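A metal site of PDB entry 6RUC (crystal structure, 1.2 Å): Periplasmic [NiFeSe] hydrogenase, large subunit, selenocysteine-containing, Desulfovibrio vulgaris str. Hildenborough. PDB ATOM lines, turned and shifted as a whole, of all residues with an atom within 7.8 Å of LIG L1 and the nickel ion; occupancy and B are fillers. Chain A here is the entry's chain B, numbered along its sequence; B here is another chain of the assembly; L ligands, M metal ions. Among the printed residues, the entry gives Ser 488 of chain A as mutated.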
ATOM      1  N   GLU A  25     -19.239  -3.703   1.657  1.00  0.00           N
ATOM      2  CA  GLU A  25     -19.622  -5.111   1.600  1.00  0.00           C
ATOM      3  C   GLU A  25     -18.490  -5.928   0.978  1.00  0.00           C
ATOM      4  O   GLU A  25     -17.867  -5.522  -0.024  1.00  0.00           O
ATOM      5  CB  GLU A  25     -20.905  -5.305   0.813  1.00  0.00           C
ATOM      6  CG  GLU A  25     -21.486  -6.717   0.837  1.00  0.00           C
ATOM      7  CD  GLU A  25     -20.653  -7.780   0.112  1.00  0.00           C
ATOM      8  OE1 GLU A  25     -20.021  -7.470  -0.926  1.00  0.00           O
ATOM      9  OE2 GLU A  25     -20.690  -8.944   0.569  1.00  0.00           O
ATOM     10  N   GLN A  69     -29.566 -14.123  -6.811  1.00  0.00           N
ATOM     11  CA  GLN A  69     -29.676 -13.124  -5.760  1.00  0.00           C
ATOM     12  C   GLN A  69     -28.655 -13.358  -4.684  1.00  0.00           C
ATOM     13  O   GLN A  69     -28.247 -12.417  -3.993  1.00  0.00           O
ATOM     14  CB  GLN A  69     -31.073 -13.116  -5.176  1.00  0.00           C
ATOM     15  CG  GLN A  69     -32.118 -12.576  -6.109  1.00  0.00           C
ATOM     16  CD  GLN A  69     -33.435 -12.418  -5.377  1.00  0.00           C
ATOM     17  OE1 GLN A  69     -33.604 -11.487  -4.565  1.00  0.00           O
ATOM     18  NE2 GLN A  69     -34.374 -13.323  -5.644  1.00  0.00           N
ATOM     19  N   ILE A  71     -25.644 -13.860  -4.950  1.00  0.00           N
ATOM     20  CA  ILE A  71     -24.422 -13.111  -5.170  1.00  0.00           C
ATOM     21  C   ILE A  71     -24.247 -12.092  -4.049  1.00  0.00           C
ATOM     22  O   ILE A  71     -23.130 -11.871  -3.589  1.00  0.00           O
ATOM     23  CB  ILE A  71     -24.418 -12.436  -6.550  1.00  0.00           C
ATOM     24  CG1 ILE A  71     -24.246 -13.520  -7.634  1.00  0.00           C
ATOM     25  CG2 ILE A  71     -23.329 -11.357  -6.630  1.00  0.00           C
ATOM     26  CD1 ILE A  71     -24.460 -13.045  -9.044  1.00  0.00           C
ATOM     27  N   CSD A  72     -25.346 -11.477  -3.615  1.00  0.00           N
ATOM     28  CA  CSD A  72     -25.240 -10.332  -2.674  1.00  0.00           C
ATOM     29  CB  CSD A  72     -24.782  -9.068  -3.400  1.00  0.00           C
ATOM     30  SG  CSD A  72     -24.676  -7.750  -2.337  1.00  0.00           S
ATOM     31  C   CSD A  72     -26.553 -10.066  -1.999  1.00  0.00           C
ATOM     32  O   CSD A  72     -27.578  -9.833  -2.671  1.00  0.00           O
ATOM     33  N   GLY A  73     -26.533 -10.083  -0.675  1.00  0.00           N
ATOM     34  CA  GLY A  73     -27.724  -9.843   0.112  1.00  0.00           C
ATOM     35  C   GLY A  73     -27.988  -8.381   0.452  1.00  0.00           C
ATOM     36  O   GLY A  73     -28.994  -8.103   1.100  1.00  0.00           O
ATOM     37  N   VAL A  74     -27.127  -7.486  -0.002  1.00  0.00           N
ATOM     38  CA  VAL A  74     -27.359  -6.043   0.061  1.00  0.00           C
ATOM     39  C   VAL A  74     -28.140  -5.558  -1.162  1.00  0.00           C
ATOM     40  O   VAL A  74     -29.086  -4.772  -1.029  1.00  0.00           O
ATOM     41  CB  VAL A  74     -26.040  -5.267   0.236  1.00  0.00           C
ATOM     42  CG1 VAL A  74     -26.299  -3.781   0.293  1.00  0.00           C
ATOM     43  CG2 VAL A  74     -25.284  -5.734   1.485  1.00  0.00           C
ATOM     44  N   CYS A  75     -27.753  -6.041  -2.366  1.00  0.00           N
ATOM     45  CA  CYS A  75     -28.411  -5.657  -3.608  1.00  0.00           C
ATOM     46  C   CYS A  75     -29.107  -6.819  -4.326  1.00  0.00           C
ATOM     47  O   CYS A  75     -29.042  -6.900  -5.560  1.00  0.00           O
ATOM     48  CB  CYS A  75     -27.404  -4.981  -4.567  1.00  0.00           C
ATOM     49  SG  CYS A  75     -26.133  -6.086  -5.195  1.00  0.00           S
ATOM     50  N   PRO A  76     -29.788  -7.723  -3.619  1.00  0.00           N
ATOM     51  CA  PRO A  76     -30.320  -8.897  -4.333  1.00  0.00           C
ATOM     52  C   PRO A  76     -31.402  -8.534  -5.329  1.00  0.00           C
ATOM     53  O   PRO A  76     -31.535  -9.221  -6.355  1.00  0.00           O
ATOM     54  CB  PRO A  76     -30.839  -9.806  -3.231  1.00  0.00           C
ATOM     55  CG  PRO A  76     -31.142  -8.880  -2.092  1.00  0.00           C
ATOM     56  CD  PRO A  76     -30.100  -7.784  -2.176  1.00  0.00           C
ATOM     57  N   ALA A  78     -31.432  -6.090  -7.356  1.00  0.00           N
ATOM     58  CA  ALA A  78     -30.805  -5.730  -8.621  1.00  0.00           C
ATOM     59  C   ALA A  78     -30.512  -6.987  -9.444  1.00  0.00           C
ATOM     60  O   ALA A  78     -30.796  -7.034 -10.658  1.00  0.00           O
ATOM     61  CB  ALA A  78     -29.534  -4.931  -8.365  1.00  0.00           C
ATOM     62  N   HIS A  79     -29.905  -8.000  -8.823  1.00  0.00           N
ATOM     63  CA  HIS A  79     -29.644  -9.258  -9.523  1.00  0.00           C
ATOM     64  C   HIS A  79     -30.935  -9.936  -9.928  1.00  0.00           C
ATOM     65  O   HIS A  79     -31.007 -10.518 -11.025  1.00  0.00           O
ATOM     66  CB  HIS A  79     -28.764 -10.161  -8.674  1.00  0.00           C
ATOM     67  CG  HIS A  79     -27.373  -9.650  -8.520  1.00  0.00           C
ATOM     68  ND1 HIS A  79     -26.478  -9.656  -9.561  1.00  0.00           N
ATOM     69  CD2 HIS A  79     -26.751  -9.074  -7.469  1.00  0.00           C
ATOM     70  CE1 HIS A  79     -25.342  -9.125  -9.159  1.00  0.00           C
ATOM     71  NE2 HIS A  79     -25.475  -8.759  -7.889  1.00  0.00           N
ATOM     72  N   ASN A 110     -35.620  -0.888  -2.514  1.00  0.00           N
ATOM     73  CA  ASN A 110     -34.267  -1.238  -2.076  1.00  0.00           C
ATOM     74  C   ASN A 110     -33.214  -0.188  -2.436  1.00  0.00           C
ATOM     75  O   ASN A 110     -32.166  -0.156  -1.780  1.00  0.00           O
ATOM     76  CB  ASN A 110     -33.792  -2.613  -2.534  1.00  0.00           C
ATOM     77  CG  ASN A 110     -32.706  -3.133  -1.623  1.00  0.00           C
ATOM     78  OD1 ASN A 110     -32.877  -3.142  -0.397  1.00  0.00           O
ATOM     79  ND2 ASN A 110     -31.561  -3.525  -2.188  1.00  0.00           N
ATOM     80  N   SER A 114     -30.669   0.837   0.383  1.00  0.00           N
ATOM     81  CA  SER A 114     -29.247   0.659   0.176  1.00  0.00           C
ATOM     82  C   SER A 114     -28.490   1.966   0.326  1.00  0.00           C
ATOM     83  O   SER A 114     -27.404   2.002   0.922  1.00  0.00           O
ATOM     84  CB  SER A 114     -29.010   0.062  -1.220  1.00  0.00           C
ATOM     85  OG  SER A 114     -27.630  -0.180  -1.452  1.00  0.00           O
ATOM     86  N   LEU A 117     -28.476   2.793   4.081  1.00  0.00           N
ATOM     87  CA  LEU A 117     -27.491   1.912   4.695  1.00  0.00           C
ATOM     88  C   LEU A 117     -26.077   2.407   4.396  1.00  0.00           C
ATOM     89  O   LEU A 117     -25.235   2.487   5.285  1.00  0.00           O
ATOM     90  CB  LEU A 117     -27.653   0.495   4.147  1.00  0.00           C
ATOM     91  CG  LEU A 117     -26.630  -0.559   4.572  1.00  0.00           C
ATOM     92  CD1 LEU A 117     -26.934  -1.049   5.980  1.00  0.00           C
ATOM     93  CD2 LEU A 117     -26.595  -1.755   3.610  1.00  0.00           C
ATOM     94  N   LEU A 122     -22.439   2.460   6.760  1.00  0.00           N
ATOM     95  CA  LEU A 122     -21.112   2.204   6.221  1.00  0.00           C
ATOM     96  C   LEU A 122     -20.246   3.469   6.263  1.00  0.00           C
ATOM     97  O   LEU A 122     -19.178   3.458   6.869  1.00  0.00           O
ATOM     98  CB  LEU A 122     -21.229   1.610   4.805  1.00  0.00           C
ATOM     99  CG  LEU A 122     -22.143   0.381   4.676  1.00  0.00           C
ATOM    100  CD1 LEU A 122     -21.997  -0.232   3.304  1.00  0.00           C
ATOM    101  CD2 LEU A 122     -21.954  -0.674   5.714  1.00  0.00           C
ATOM    102  N   ALA A 417     -28.051  -1.340 -10.596  1.00  0.00           N
ATOM    103  CA  ALA A 417     -28.086  -1.629  -9.183  1.00  0.00           C
ATOM    104  C   ALA A 417     -27.779  -0.350  -8.422  1.00  0.00           C
ATOM    105  O   ALA A 417     -27.255   0.605  -9.009  1.00  0.00           O
ATOM    106  CB  ALA A 417     -27.031  -2.683  -8.848  1.00  0.00           C
ATOM    107  N   PRO A 418     -28.088  -0.288  -7.130  1.00  0.00           N
ATOM    108  CA  PRO A 418     -27.750   0.936  -6.370  1.00  0.00           C
ATOM    109  C   PRO A 418     -26.303   1.401  -6.506  1.00  0.00           C
ATOM    110  O   PRO A 418     -26.045   2.606  -6.419  1.00  0.00           O
ATOM    111  CB  PRO A 418     -28.104   0.548  -4.936  1.00  0.00           C
ATOM    112  CG  PRO A 418     -29.247  -0.444  -5.097  1.00  0.00           C
ATOM    113  CD  PRO A 418     -28.858  -1.250  -6.316  1.00  0.00           C
ATOM    114  N   ARG A 419     -25.361   0.491  -6.726  1.00  0.00           N
ATOM    115  CA  ARG A 419     -23.953   0.847  -6.878  1.00  0.00           C
ATOM    116  C   ARG A 419     -23.512   1.036  -8.320  1.00  0.00           C
ATOM    117  O   ARG A 419     -22.368   1.464  -8.539  1.00  0.00           O
ATOM    118  CB  ARG A 419     -23.096  -0.210  -6.190  1.00  0.00           C
ATOM    119  CG  ARG A 419     -23.277  -0.132  -4.685  1.00  0.00           C
ATOM    120  CD  ARG A 419     -22.973  -1.420  -3.936  1.00  0.00           C
ATOM    121  NE  ARG A 419     -23.295  -1.178  -2.546  1.00  0.00           N
ATOM    122  CZ  ARG A 419     -24.530  -1.168  -2.050  1.00  0.00           C
ATOM    123  NH1 ARG A 419     -25.573  -1.545  -2.786  1.00  0.00           N
ATOM    124  NH2 ARG A 419     -24.736  -0.807  -0.795  1.00  0.00           N
ATOM    125  N   SER A 440     -21.213  -6.741 -13.148  1.00  0.00           N
ATOM    126  CA  SER A 440     -21.899  -6.048 -12.056  1.00  0.00           C
ATOM    127  C   SER A 440     -21.270  -4.681 -11.748  1.00  0.00           C
ATOM    128  O   SER A 440     -20.235  -4.287 -12.294  1.00  0.00           O
ATOM    129  CB  SER A 440     -21.834  -6.920 -10.815  1.00  0.00           C
ATOM    130  OG  SER A 440     -20.484  -7.133 -10.479  1.00  0.00           O
ATOM    131  N   ALA A 441     -21.894  -3.955 -10.817  1.00  0.00           N
ATOM    132  CA  ALA A 441     -21.513  -2.565 -10.567  1.00  0.00           C
ATOM    133  C   ALA A 441     -20.121  -2.460  -9.978  1.00  0.00           C
ATOM    134  O   ALA A 441     -19.253  -1.739 -10.499  1.00  0.00           O
ATOM    135  CB  ALA A 441     -22.523  -1.913  -9.631  1.00  0.00           C
ATOM    136  N   SER A 442     -19.876  -3.155  -8.868  1.00  0.00           N
ATOM    137  CA  SER A 442     -18.571  -3.043  -8.233  1.00  0.00           C
ATOM    138  C   SER A 442     -17.483  -3.753  -9.029  1.00  0.00           C
ATOM    139  O   SER A 442     -16.296  -3.530  -8.760  1.00  0.00           O
ATOM    140  CB  SER A 442     -18.623  -3.535  -6.787  1.00  0.00           C
ATOM    141  OG  SER A 442     -19.418  -2.684  -5.984  1.00  0.00           O
ATOM    142  N   ASP A 484     -19.110   3.044  -2.442  1.00  0.00           N
ATOM    143  CA  ASP A 484     -20.034   2.037  -1.936  1.00  0.00           C
ATOM    144  C   ASP A 484     -19.712   0.649  -2.486  1.00  0.00           C
ATOM    145  O   ASP A 484     -20.558  -0.003  -3.097  1.00  0.00           O
ATOM    146  CB  ASP A 484     -21.460   2.461  -2.281  1.00  0.00           C
ATOM    147  CG  ASP A 484     -22.568   1.693  -1.580  1.00  0.00           C
ATOM    148  OD1 ASP A 484     -22.348   0.826  -0.712  1.00  0.00           O
ATOM    149  OD2 ASP A 484     -23.732   2.023  -1.946  1.00  0.00           O
ATOM    150  N   PRO A 485     -18.465   0.153  -2.273  1.00  0.00           N
ATOM    151  CA  PRO A 485     -18.101  -1.146  -2.832  1.00  0.00           C
ATOM    152  C   PRO A 485     -18.857  -2.334  -2.270  1.00  0.00           C
ATOM    153  O   PRO A 485     -19.187  -2.378  -1.084  1.00  0.00           O
ATOM    154  CB  PRO A 485     -16.621  -1.321  -2.434  1.00  0.00           C
ATOM    155  CG  PRO A 485     -16.154   0.013  -2.089  1.00  0.00           C
ATOM    156  CD  PRO A 485     -17.337   0.754  -1.540  1.00  0.00           C
ATOM    157  N   SEC A 486     -19.202  -3.303  -3.117  1.00  0.00           N
ATOM    158  CA  SEC A 486     -19.597  -4.602  -2.599  1.00  0.00           C
ATOM    159  CB  SEC A 486     -21.083  -4.807  -2.343  1.00  0.00           C
ATOM    160 SE   SEC A 486     -22.301  -4.558  -3.826  1.00  0.00          SE
ATOM    161  C   SEC A 486     -18.915  -5.645  -3.431  1.00  0.00           C
ATOM    162  O   SEC A 486     -19.290  -5.930  -4.569  1.00  0.00           O
ATOM    163  N   LEU A 487     -17.876  -6.215  -2.833  1.00  0.00           N
ATOM    164  CA  LEU A 487     -16.957  -7.116  -3.525  1.00  0.00           C
ATOM    165  C   LEU A 487     -17.592  -8.447  -3.826  1.00  0.00           C
ATOM    166  O   LEU A 487     -17.178  -9.111  -4.781  1.00  0.00           O
ATOM    167  CB  LEU A 487     -15.619  -7.274  -2.787  1.00  0.00           C
ATOM    168  CG  LEU A 487     -14.559  -6.226  -3.167  1.00  0.00           C
ATOM    169  CD1 LEU A 487     -14.133  -6.369  -4.618  1.00  0.00           C
ATOM    170  CD2 LEU A 487     -15.066  -4.788  -2.920  1.00  0.00           C
ATOM    171  N   SER A 488     -18.619  -8.846  -3.072  1.00  0.00           N
ATOM    172  CA  SER A 488     -19.330 -10.067  -3.415  1.00  0.00           C
ATOM    173  C   SER A 488     -20.028  -9.942  -4.761  1.00  0.00           C
ATOM    174  O   SER A 488     -19.995 -10.870  -5.587  1.00  0.00           O
ATOM    175  CB  SER A 488     -20.285 -10.452  -2.290  1.00  0.00           C
ATOM    176  OG  SER A 488     -19.569 -10.611  -1.061  1.00  0.00           O
ATOM    177  N   CYS A 489     -20.625  -8.777  -5.034  1.00  0.00           N
ATOM    178  CA  CYS A 489     -21.112  -8.483  -6.390  1.00  0.00           C
ATOM    179  C   CYS A 489     -19.994  -8.489  -7.403  1.00  0.00           C
ATOM    180  O   CYS A 489     -20.161  -8.984  -8.531  1.00  0.00           O
ATOM    181  CB  CYS A 489     -21.776  -7.103  -6.445  1.00  0.00           C
ATOM    182  SG  CYS A 489     -23.496  -7.097  -5.980  1.00  0.00           S
ATOM    183  N   ALA A 490     -18.845  -7.874  -7.070  1.00  0.00           N
ATOM    184  CA  ALA A 490     -17.779  -7.688  -8.052  1.00  0.00           C
ATOM    185  C   ALA A 490     -17.230  -9.028  -8.519  1.00  0.00           C
ATOM    186  O   ALA A 490     -16.902  -9.189  -9.705  1.00  0.00           O
ATOM    187  CB  ALA A 490     -16.657  -6.839  -7.458  1.00  0.00           C
ATOM    188  N   CYS B  18     -22.819 -13.759   1.330  1.00  0.00           N
ATOM    189  CA  CYS B  18     -23.299 -12.686   0.468  1.00  0.00           C
ATOM    190  C   CYS B  18     -23.666 -11.438   1.267  1.00  0.00           C
ATOM    191  O   CYS B  18     -24.154 -10.470   0.679  1.00  0.00           O
ATOM    192  CB  CYS B  18     -24.523 -13.141  -0.343  1.00  0.00           C
ATOM    193  SG  CYS B  18     -26.083 -13.204   0.621  1.00  0.00           S
ATOM    194  N   THR B  19     -23.457 -11.457   2.579  1.00  0.00           N
ATOM    195  CA  THR B  19     -23.793 -10.378   3.514  1.00  0.00           C
ATOM    196  C   THR B  19     -25.307 -10.344   3.811  1.00  0.00           C
ATOM    197  O   THR B  19     -25.759  -9.570   4.656  1.00  0.00           O
ATOM    198  CB  THR B  19     -23.160  -9.038   3.103  1.00  0.00           C
ATOM    199  OG1 THR B  19     -21.743  -9.264   2.982  1.00  0.00           O
ATOM    200  CG2 THR B  19     -23.356  -7.939   4.139  1.00  0.00           C
HETATM  201  S1  LIG L   1     -24.196  -4.397  -2.837  1.00  0.00           S
HETATM  202 FE1  LG2 L   2     -24.460  -5.037  -6.284  1.00  0.00          FE
HETATM  203  C1  LG2 L   2     -22.827  -4.276  -6.581  1.00  0.00           C
HETATM  204  N1  LG2 L   2     -21.797  -3.728  -6.713  1.00  0.00           N
HETATM  205  C2  LG2 L   2     -25.212  -3.397  -5.997  1.00  0.00           C
HETATM  206  N2  LG2 L   2     -25.681  -2.330  -5.888  1.00  0.00           N
HETATM  207  C3  LG2 L   2     -24.684  -5.115  -8.088  1.00  0.00           C
HETATM  208  O1  LG2 L   2     -24.756  -5.110  -9.219  1.00  0.00           O
HETATM  209 NI    NI M   1     -24.155  -6.089  -4.077  1.00  0.00          NI
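S1 of LIG L1 is covalently linked to SE of SEC 486, at 2.1 Å.
The guanidinium group (NH1) of Arg 419 lies close to a sulfur (S1) of LIG L1 (3.2 Å).
An iron atom (FE1) of LG2 L2 is bound by the side-chain sulfur of Cys 489, 2.3 Å away.
The side-chain sulfur (SG) of Cys 75 binds an iron atom (FE1) of LG2 L2 (2.3 Å).
A nitrogen (N2) of LG2 L2 lies within hydrogen-bond range of the backbone NH (N) of Arg 419 (3.0 Å).
A nitrogen (N2) of LG2 L2 sits at hydrogen-bond distance from the guanidinium group of Arg 419 (3.2 Å).
A nitrogen (N1) of LG2 L2 sits at hydrogen-bond distance from the backbone NH (N) of Ser 442 (2.9 Å).
The side-chain hydroxyl (OG) of Ser 442 lies within hydrogen-bond range of a nitrogen (N1) of LG2 L2 (2.7 Å).
N of Ala 441 lies within hydrogen-bond range of O1 of LG2 L2 (3.5 Å).
OG of Ser 442 sits at hydrogen-bond distance from N of SEC 486, at 2.9 Å.
The side-chain sulfur (SG) of Cys 489 lies close to a ring nitrogen (NE2) of His 79 (3.2 Å).
O of Cys 489 is in hydrogen-bond range of OG of Ser 440 (2.7 Å).
The backbone NH of Val 74 lies close to SG of CSD 72, 3.4 Å away.
NH1 of Arg 419 lies within hydrogen-bond range of OG of Ser 114 (2.8 Å).
NE of Arg 419 is in salt-bridge range of OD1 of Asp 484 (2.9 Å).
The side-chain amide nitrogen (ND2) of Asn 110 is in hydrogen-bond range of the backbone carbonyl oxygen (O) of Val 74.
Merely in contact with LIG L1: Val 74.
Of the 29 residues printed, 5 come within 4 Å of LIG L1.
Within 4 Å of the nickel ion: CSD 72, Cys 75, SEC 486 and Cys 489.
The nearest printed residue that does not touch the nickel ion is Val 74 (4.8 Å).
The nickel ion is bound by a sulfur (S1) of LIG L1, the side-chain sulfur of Cys 489, the side-chain sulfur of Cys 75, SE of SEC 486 and SG of CSD 72.
The nickel ion has five donor atoms within binding distance.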
